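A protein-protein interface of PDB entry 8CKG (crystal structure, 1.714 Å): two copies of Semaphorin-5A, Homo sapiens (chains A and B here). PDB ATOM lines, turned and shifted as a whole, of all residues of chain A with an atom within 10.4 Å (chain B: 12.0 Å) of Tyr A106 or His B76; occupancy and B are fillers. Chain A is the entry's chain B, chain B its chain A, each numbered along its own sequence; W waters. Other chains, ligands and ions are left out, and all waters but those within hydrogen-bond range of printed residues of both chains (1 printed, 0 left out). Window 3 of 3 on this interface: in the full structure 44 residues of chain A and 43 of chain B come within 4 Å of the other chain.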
ATOM      1  N   GLU A 103     -29.857  25.141 -14.270  1.00  0.00           N
ATOM      2  CA  GLU A 103     -28.870  24.152 -13.871  1.00  0.00           C
ATOM      3  C   GLU A 103     -28.372  23.439 -15.116  1.00  0.00           C
ATOM      4  O   GLU A 103     -29.171  23.075 -15.986  1.00  0.00           O
ATOM      5  CB  GLU A 103     -29.436  23.143 -12.863  1.00  0.00           C
ATOM      6  CG  GLU A 103     -28.358  22.249 -12.254  1.00  0.00           C
ATOM      7  CD  GLU A 103     -28.905  21.083 -11.431  1.00  0.00           C
ATOM      8  OE1 GLU A 103     -30.148  20.914 -11.372  1.00  0.00           O
ATOM      9  OE2 GLU A 103     -28.083  20.340 -10.832  1.00  0.00           O
ATOM     10  N   MET A 104     -27.059  23.265 -15.216  1.00  0.00           N
ATOM     11  CA  MET A 104     -26.440  22.455 -16.262  1.00  0.00           C
ATOM     12  C   MET A 104     -25.729  21.239 -15.676  1.00  0.00           C
ATOM     13  O   MET A 104     -25.347  21.213 -14.500  1.00  0.00           O
ATOM     14  CB  MET A 104     -25.433  23.272 -17.076  1.00  0.00           C
ATOM     15  CG  MET A 104     -26.060  24.439 -17.819  1.00  0.00           C
ATOM     16  SD  MET A 104     -24.865  25.388 -18.784  1.00  0.00           S
ATOM     17  CE  MET A 104     -24.225  24.123 -19.841  1.00  0.00           C
ATOM     18  N   ARG A 105     -25.532  20.221 -16.515  1.00  0.00           N
ATOM     19  CA  ARG A 105     -24.708  19.083 -16.146  1.00  0.00           C
ATOM     20  C   ARG A 105     -23.805  18.717 -17.314  1.00  0.00           C
ATOM     21  O   ARG A 105     -24.223  18.762 -18.474  1.00  0.00           O
ATOM     22  CB  ARG A 105     -25.563  17.888 -15.711  1.00  0.00           C
ATOM     23  CG  ARG A 105     -26.501  17.320 -16.780  1.00  0.00           C
ATOM     24  CD  ARG A 105     -27.351  16.227 -16.164  1.00  0.00           C
ATOM     25  NE  ARG A 105     -28.211  15.557 -17.134  1.00  0.00           N
ATOM     26  CZ  ARG A 105     -29.098  14.628 -16.803  1.00  0.00           C
ATOM     27  NH1 ARG A 105     -29.278  14.267 -15.540  1.00  0.00           N
ATOM     28  NH2 ARG A 105     -29.824  14.056 -17.759  1.00  0.00           N
ATOM     29  N   TYR A 106     -22.560  18.385 -16.996  1.00  0.00           N
ATOM     30  CA  TYR A 106     -21.592  17.905 -17.975  1.00  0.00           C
ATOM     31  C   TYR A 106     -21.865  16.447 -18.317  1.00  0.00           C
ATOM     32  O   TYR A 106     -22.021  15.612 -17.418  1.00  0.00           O
ATOM     33  CB  TYR A 106     -20.186  18.055 -17.405  1.00  0.00           C
ATOM     34  CG  TYR A 106     -19.061  17.702 -18.347  1.00  0.00           C
ATOM     35  CD1 TYR A 106     -19.003  18.232 -19.631  1.00  0.00           C
ATOM     36  CD2 TYR A 106     -18.042  16.860 -17.932  1.00  0.00           C
ATOM     37  CE1 TYR A 106     -17.954  17.908 -20.486  1.00  0.00           C
ATOM     38  CE2 TYR A 106     -16.993  16.538 -18.765  1.00  0.00           C
ATOM     39  CZ  TYR A 106     -16.947  17.064 -20.039  1.00  0.00           C
ATOM     40  OH  TYR A 106     -15.889  16.721 -20.860  1.00  0.00           O
ATOM     41  N   CYS A 107     -21.916  16.130 -19.616  1.00  0.00           N
ATOM     42  CA  CYS A 107     -22.173  14.767 -20.064  1.00  0.00           C
ATOM     43  C   CYS A 107     -20.927  14.013 -20.518  1.00  0.00           C
ATOM     44  O   CYS A 107     -21.061  12.904 -21.057  1.00  0.00           O
ATOM     45  CB  CYS A 107     -23.199  14.779 -21.192  1.00  0.00           C
ATOM     46  SG  CYS A 107     -24.720  15.566 -20.673  1.00  0.00           S
ATOM     47  N   SER A 108     -19.726  14.576 -20.296  1.00  0.00           N
ATOM     48  CA  SER A 108     -18.447  13.973 -20.669  1.00  0.00           C
ATOM     49  C   SER A 108     -18.282  14.034 -22.180  1.00  0.00           C
ATOM     50  O   SER A 108     -19.205  14.445 -22.896  1.00  0.00           O
ATOM     51  CB  SER A 108     -18.309  12.516 -20.177  1.00  0.00           C
ATOM     52  OG  SER A 108     -18.697  11.584 -21.178  1.00  0.00           O
ATOM     53  N   SER A 109     -17.111  13.626 -22.678  1.00  0.00           N
ATOM     54  CA  SER A 109     -16.880  13.685 -24.118  1.00  0.00           C
ATOM     55  C   SER A 109     -17.707  12.652 -24.883  1.00  0.00           C
ATOM     56  O   SER A 109     -17.912  12.824 -26.088  1.00  0.00           O
ATOM     57  CB  SER A 109     -15.387  13.530 -24.423  1.00  0.00           C
ATOM     58  OG  SER A 109     -14.786  12.499 -23.683  1.00  0.00           O
ATOM     59  N   ASP A 110     -18.214  11.601 -24.222  1.00  0.00           N
ATOM     60  CA  ASP A 110     -19.084  10.663 -24.929  1.00  0.00           C
ATOM     61  C   ASP A 110     -20.526  11.172 -25.042  1.00  0.00           C
ATOM     62  O   ASP A 110     -21.323  10.586 -25.781  1.00  0.00           O
ATOM     63  CB  ASP A 110     -19.018   9.266 -24.275  1.00  0.00           C
ATOM     64  CG  ASP A 110     -19.757   9.178 -22.926  1.00  0.00           C
ATOM     65  OD1 ASP A 110     -20.565  10.064 -22.574  1.00  0.00           O
ATOM     66  OD2 ASP A 110     -19.526   8.189 -22.199  1.00  0.00           O
ATOM     67  N   GLY A 111     -20.884  12.236 -24.323  1.00  0.00           N
ATOM     68  CA  GLY A 111     -22.161  12.894 -24.506  1.00  0.00           C
ATOM     69  C   GLY A 111     -23.344  12.281 -23.779  1.00  0.00           C
ATOM     70  O   GLY A 111     -24.457  12.804 -23.905  1.00  0.00           O
ATOM     71  N   THR A 112     -23.153  11.193 -23.023  1.00  0.00           N
ATOM     72  CA  THR A 112     -24.271  10.565 -22.314  1.00  0.00           C
ATOM     73  C   THR A 112     -23.979  10.182 -20.867  1.00  0.00           C
ATOM     74  O   THR A 112     -24.921  10.180 -20.065  1.00  0.00           O
ATOM     75  CB  THR A 112     -24.764   9.301 -23.047  1.00  0.00           C
ATOM     76  OG1 THR A 112     -23.664   8.422 -23.284  1.00  0.00           O
ATOM     77  CG2 THR A 112     -25.417   9.653 -24.371  1.00  0.00           C
ATOM     78  N   SER A 113     -22.735   9.860 -20.491  1.00  0.00           N
ATOM     79  CA  SER A 113     -22.462   9.358 -19.141  1.00  0.00           C
ATOM     80  C   SER A 113     -22.759  10.417 -18.087  1.00  0.00           C
ATOM     81  O   SER A 113     -22.282  11.556 -18.173  1.00  0.00           O
ATOM     82  CB  SER A 113     -21.006   8.907 -19.024  1.00  0.00           C
ATOM     83  OG  SER A 113     -20.730   7.822 -19.902  1.00  0.00           O
ATOM     84  N   GLY A 114     -23.524  10.025 -17.067  1.00  0.00           N
ATOM     85  CA  GLY A 114     -24.030  10.950 -16.076  1.00  0.00           C
ATOM     86  C   GLY A 114     -25.237  11.736 -16.523  1.00  0.00           C
ATOM     87  O   GLY A 114     -25.804  12.490 -15.717  1.00  0.00           O
ATOM     88  N   CYS A 115     -25.638  11.615 -17.792  1.00  0.00           N
ATOM     89  CA  CYS A 115     -26.801  12.326 -18.288  1.00  0.00           C
ATOM     90  C   CYS A 115     -27.829  11.263 -18.616  1.00  0.00           C
ATOM     91  O   CYS A 115     -28.510  10.767 -17.699  1.00  0.00           O
ATOM     92  CB  CYS A 115     -26.399  13.259 -19.445  1.00  0.00           C
ATOM     93  SG  CYS A 115     -25.241  14.622 -18.907  1.00  0.00           S
ATOM     94  N   SER A 116     -27.947  10.811 -19.872  1.00  0.00           N
ATOM     95  CA  SER A 116     -28.957   9.806 -20.178  1.00  0.00           C
ATOM     96  C   SER A 116     -28.500   8.385 -19.868  1.00  0.00           C
ATOM     97  O   SER A 116     -29.336   7.470 -19.839  1.00  0.00           O
ATOM     98  CB  SER A 116     -29.385   9.918 -21.643  1.00  0.00           C
ATOM     99  OG  SER A 116     -28.290   9.652 -22.499  1.00  0.00           O
ATOM    100  N   THR A 117     -27.210   8.164 -19.621  1.00  0.00           N
ATOM    101  CA  THR A 117     -26.717   6.819 -19.356  1.00  0.00           C
ATOM    102  C   THR A 117     -25.885   6.825 -18.083  1.00  0.00           C
ATOM    103  O   THR A 117     -25.272   7.832 -17.726  1.00  0.00           O
ATOM    104  CB  THR A 117     -25.855   6.252 -20.523  1.00  0.00           C
ATOM    105  OG1 THR A 117     -24.614   6.972 -20.602  1.00  0.00           O
ATOM    106  CG2 THR A 117     -26.588   6.346 -21.853  1.00  0.00           C
ATOM    107  N   TRP B  65     -34.442  17.825 -18.642  1.00  0.00           N
ATOM    108  CA  TRP B  65     -33.097  18.111 -19.119  1.00  0.00           C
ATOM    109  C   TRP B  65     -33.116  18.178 -20.636  1.00  0.00           C
ATOM    110  O   TRP B  65     -33.751  17.352 -21.297  1.00  0.00           O
ATOM    111  CB  TRP B  65     -32.122  17.031 -18.660  1.00  0.00           C
ATOM    112  CG  TRP B  65     -31.775  17.020 -17.198  1.00  0.00           C
ATOM    113  CD1 TRP B  65     -32.238  16.143 -16.256  1.00  0.00           C
ATOM    114  CD2 TRP B  65     -30.856  17.885 -16.522  1.00  0.00           C
ATOM    115  NE1 TRP B  65     -31.668  16.413 -15.035  1.00  0.00           N
ATOM    116  CE2 TRP B  65     -30.808  17.471 -15.170  1.00  0.00           C
ATOM    117  CE3 TRP B  65     -30.063  18.960 -16.927  1.00  0.00           C
ATOM    118  CZ2 TRP B  65     -30.019  18.110 -14.222  1.00  0.00           C
ATOM    119  CZ3 TRP B  65     -29.271  19.593 -15.981  1.00  0.00           C
ATOM    120  CH2 TRP B  65     -29.255  19.167 -14.646  1.00  0.00           C
ATOM    121  N   THR B  66     -32.442  19.175 -21.197  1.00  0.00           N
ATOM    122  CA  THR B  66     -32.409  19.366 -22.641  1.00  0.00           C
ATOM    123  C   THR B  66     -30.973  19.660 -23.054  1.00  0.00           C
ATOM    124  O   THR B  66     -30.205  20.186 -22.254  1.00  0.00           O
ATOM    125  CB  THR B  66     -33.336  20.521 -23.071  1.00  0.00           C
ATOM    126  OG1 THR B  66     -32.920  21.740 -22.436  1.00  0.00           O
ATOM    127  CG2 THR B  66     -34.792  20.231 -22.682  1.00  0.00           C
ATOM    128  N   PRO B  67     -30.580  19.335 -24.276  1.00  0.00           N
ATOM    129  CA  PRO B  67     -29.170  19.525 -24.648  1.00  0.00           C
ATOM    130  C   PRO B  67     -28.824  20.986 -24.914  1.00  0.00           C
ATOM    131  O   PRO B  67     -29.676  21.803 -25.271  1.00  0.00           O
ATOM    132  CB  PRO B  67     -29.015  18.676 -25.921  1.00  0.00           C
ATOM    133  CG  PRO B  67     -30.425  18.257 -26.326  1.00  0.00           C
ATOM    134  CD  PRO B  67     -31.406  18.944 -25.428  1.00  0.00           C
ATOM    135  N   VAL B  68     -27.543  21.307 -24.714  1.00  0.00           N
ATOM    136  CA  VAL B  68     -26.994  22.615 -25.076  1.00  0.00           C
ATOM    137  C   VAL B  68     -25.989  22.397 -26.195  1.00  0.00           C
ATOM    138  O   VAL B  68     -26.172  22.894 -27.303  1.00  0.00           O
ATOM    139  CB  VAL B  68     -26.308  23.341 -23.897  1.00  0.00           C
ATOM    140  CG1 VAL B  68     -26.133  24.818 -24.225  1.00  0.00           C
ATOM    141  CG2 VAL B  68     -27.076  23.177 -22.616  1.00  0.00           C
ATOM    142  N   HIS B  76     -22.087  17.342 -24.961  1.00  0.00           N
ATOM    143  CA  HIS B  76     -21.233  17.866 -23.907  1.00  0.00           C
ATOM    144  C   HIS B  76     -22.060  18.278 -22.667  1.00  0.00           C
ATOM    145  O   HIS B  76     -21.741  17.831 -21.560  1.00  0.00           O
ATOM    146  CB  HIS B  76     -20.392  19.040 -24.429  1.00  0.00           C
ATOM    147  N   TYR B  77     -23.122  19.086 -22.825  1.00  0.00           N
ATOM    148  CA  TYR B  77     -23.878  19.584 -21.682  1.00  0.00           C
ATOM    149  C   TYR B  77     -25.377  19.505 -21.911  1.00  0.00           C
ATOM    150  O   TYR B  77     -25.856  19.651 -23.031  1.00  0.00           O
ATOM    151  CB  TYR B  77     -23.554  21.045 -21.360  1.00  0.00           C
ATOM    152  CG  TYR B  77     -22.157  21.260 -20.873  1.00  0.00           C
ATOM    153  CD1 TYR B  77     -21.865  21.277 -19.504  1.00  0.00           C
ATOM    154  CD2 TYR B  77     -21.127  21.453 -21.770  1.00  0.00           C
ATOM    155  CE1 TYR B  77     -20.569  21.472 -19.061  1.00  0.00           C
ATOM    156  CE2 TYR B  77     -19.837  21.647 -21.342  1.00  0.00           C
ATOM    157  CZ  TYR B  77     -19.561  21.661 -19.989  1.00  0.00           C
ATOM    158  OH  TYR B  77     -18.266  21.856 -19.582  1.00  0.00           O
ATOM    159  N   GLU B  78     -26.112  19.326 -20.818  1.00  0.00           N
ATOM    160  CA  GLU B  78     -27.560  19.458 -20.777  1.00  0.00           C
ATOM    161  C   GLU B  78     -27.915  20.530 -19.758  1.00  0.00           C
ATOM    162  O   GLU B  78     -27.119  20.852 -18.866  1.00  0.00           O
ATOM    163  CB  GLU B  78     -28.242  18.127 -20.409  1.00  0.00           C
ATOM    164  CG  GLU B  78     -28.033  17.035 -21.437  1.00  0.00           C
ATOM    165  CD  GLU B  78     -28.652  15.709 -21.042  1.00  0.00           C
ATOM    166  OE1 GLU B  78     -28.988  15.546 -19.851  1.00  0.00           O
ATOM    167  OE2 GLU B  78     -28.791  14.828 -21.921  1.00  0.00           O
ATOM    168  N   GLN B  79     -29.120  21.084 -19.895  1.00  0.00           N
ATOM    169  CA  GLN B  79     -29.574  22.167 -19.034  1.00  0.00           C
ATOM    170  C   GLN B  79     -31.055  21.992 -18.728  1.00  0.00           C
ATOM    171  O   GLN B  79     -31.794  21.357 -19.495  1.00  0.00           O
ATOM    172  CB  GLN B  79     -29.311  23.539 -19.686  1.00  0.00           C
ATOM    173  CG  GLN B  79     -30.285  23.880 -20.805  1.00  0.00           C
ATOM    174  CD  GLN B  79     -29.881  25.135 -21.574  1.00  0.00           C
ATOM    175  OE1 GLN B  79     -29.144  25.979 -21.062  1.00  0.00           O
ATOM    176  NE2 GLN B  79     -30.357  25.253 -22.810  1.00  0.00           N
ATOM    177  N   ARG B  80     -31.479  22.562 -17.595  1.00  0.00           N
ATOM    178  CA  ARG B  80     -32.890  22.655 -17.222  1.00  0.00           C
ATOM    179  C   ARG B  80     -33.132  23.974 -16.491  1.00  0.00           C
ATOM    180  O   ARG B  80     -32.196  24.663 -16.062  1.00  0.00           O
ATOM    181  CB  ARG B  80     -33.324  21.457 -16.378  1.00  0.00           C
ATOM    182  CG  ARG B  80     -32.515  21.267 -15.091  1.00  0.00           C
ATOM    183  CD  ARG B  80     -33.018  20.053 -14.319  1.00  0.00           C
ATOM    184  NE  ARG B  80     -32.308  19.851 -13.053  1.00  0.00           N
ATOM    185  CZ  ARG B  80     -32.614  18.898 -12.180  1.00  0.00           C
ATOM    186  NH1 ARG B  80     -33.610  18.057 -12.406  1.00  0.00           N
ATOM    187  NH2 ARG B  80     -31.910  18.793 -11.048  1.00  0.00           N
HETATM  188  O   HOH W   1     -27.227  12.425 -22.538  1.00  0.00           O
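Of the 15 printed residues of chain A, 6 touch a printed residue of chain B.
Hydrophobic or aromatic side chains of chain A within 4 Å of the printed part of chain B: Met A104 and Tyr A106.
Of the 9 printed residues of chain B, 6 touch a printed residue of chain A.
Hydrophobic or aromatic side chains of chain B that line the printed part of chain A: Trp B65 and Tyr B77.
Among the printed residues, 15 pairs touch across the chains.
Among the printed residues, Asp or Glu carboxylates within 4 Å of a Lys or Arg side-chain nitrogen of the other chain: Glu A103 with Arg B80 (2.8 Å) and Arg A105 with Glu B78 (2.7 Å).
Among the printed residues, merely in contact across the chains: Glu A103 with Trp B65, Glu A103 with Gln B79, Met A104 with Trp B65, Met A104 with Tyr B77, Met A104 with Glu B78, Met A104 with Gln B79, Arg A105 with Tyr B77, Tyr A106 with His B76, Tyr A106 with Tyr B77, Cys A107 with Glu B78 and Cys A115 with Glu B78.
O of Thr B66 lies within hydrogen-bond range of N of Gln B79 (2.7 Å).
O of Tyr B77 sits at hydrogen-bond distance from N of Val B68 (2.9 Å).
SG of Cys A115 is in hydrogen-bond range of NE of Arg A105 (3.6 Å).
O of Cys A107 sits at hydrogen-bond distance from N of Thr A112 (3.3 Å).
The side-chain sulfur (SG) of Cys A115 forms a disulfide with the side-chain sulfur (SG) of Cys A107 (2.1 Å).
No position is printed for both chains.
His B76 touches just these residues of chain A: Tyr A106 and Cys A107.
No residue of chain B comes within 4 Å of Ser A108.
Ser A109 touches none of the printed residues of chain B.
No residue of chain B comes within 4 Å of Gly A111.
No residue of chain B comes within 4 Å of Gly A114.
Printed residues of chain A within 4 Å of Tyr B77: Met A104 (3.5 Å), Arg A105 (3.3 Å) and Tyr A106 (3.5 Å).
Of the printed residues of chain A, Arg B80 touches Glu A103.
Of the printed residues of chain A, Gln B79 touches Glu A103 (3.2 Å) and Met A104 (3.9 Å).
Of the printed residues of chain A, Glu B78 touches Met A104, Arg A105, Cys A107 and Cys A115.
Pro B67 touches none of the printed residues of chain A.
The nearest printed residue of chain A that does not touch Glu B78 is Glu A103 (4.2 Å).
The backbone carbonyl oxygen of His B76 lies within hydrogen-bond range of the backbone NH of Cys A107, at 2.6 Å.
The guanidinium group (NH2) of Arg A105 is in salt-bridge range of the side-chain carboxylate (OE1) of Glu B78.
OE1 of Glu A103 lies within salt-bridge range of NH2 of Arg B80 (2.8 Å).
NH1 of Arg A105 sits close to NE1 of Trp B65 (3.3 Å).
Water W1 lies within hydrogen-bond range of OE2 of Glu B78, OG of Ser A116 and O of Gly A111.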
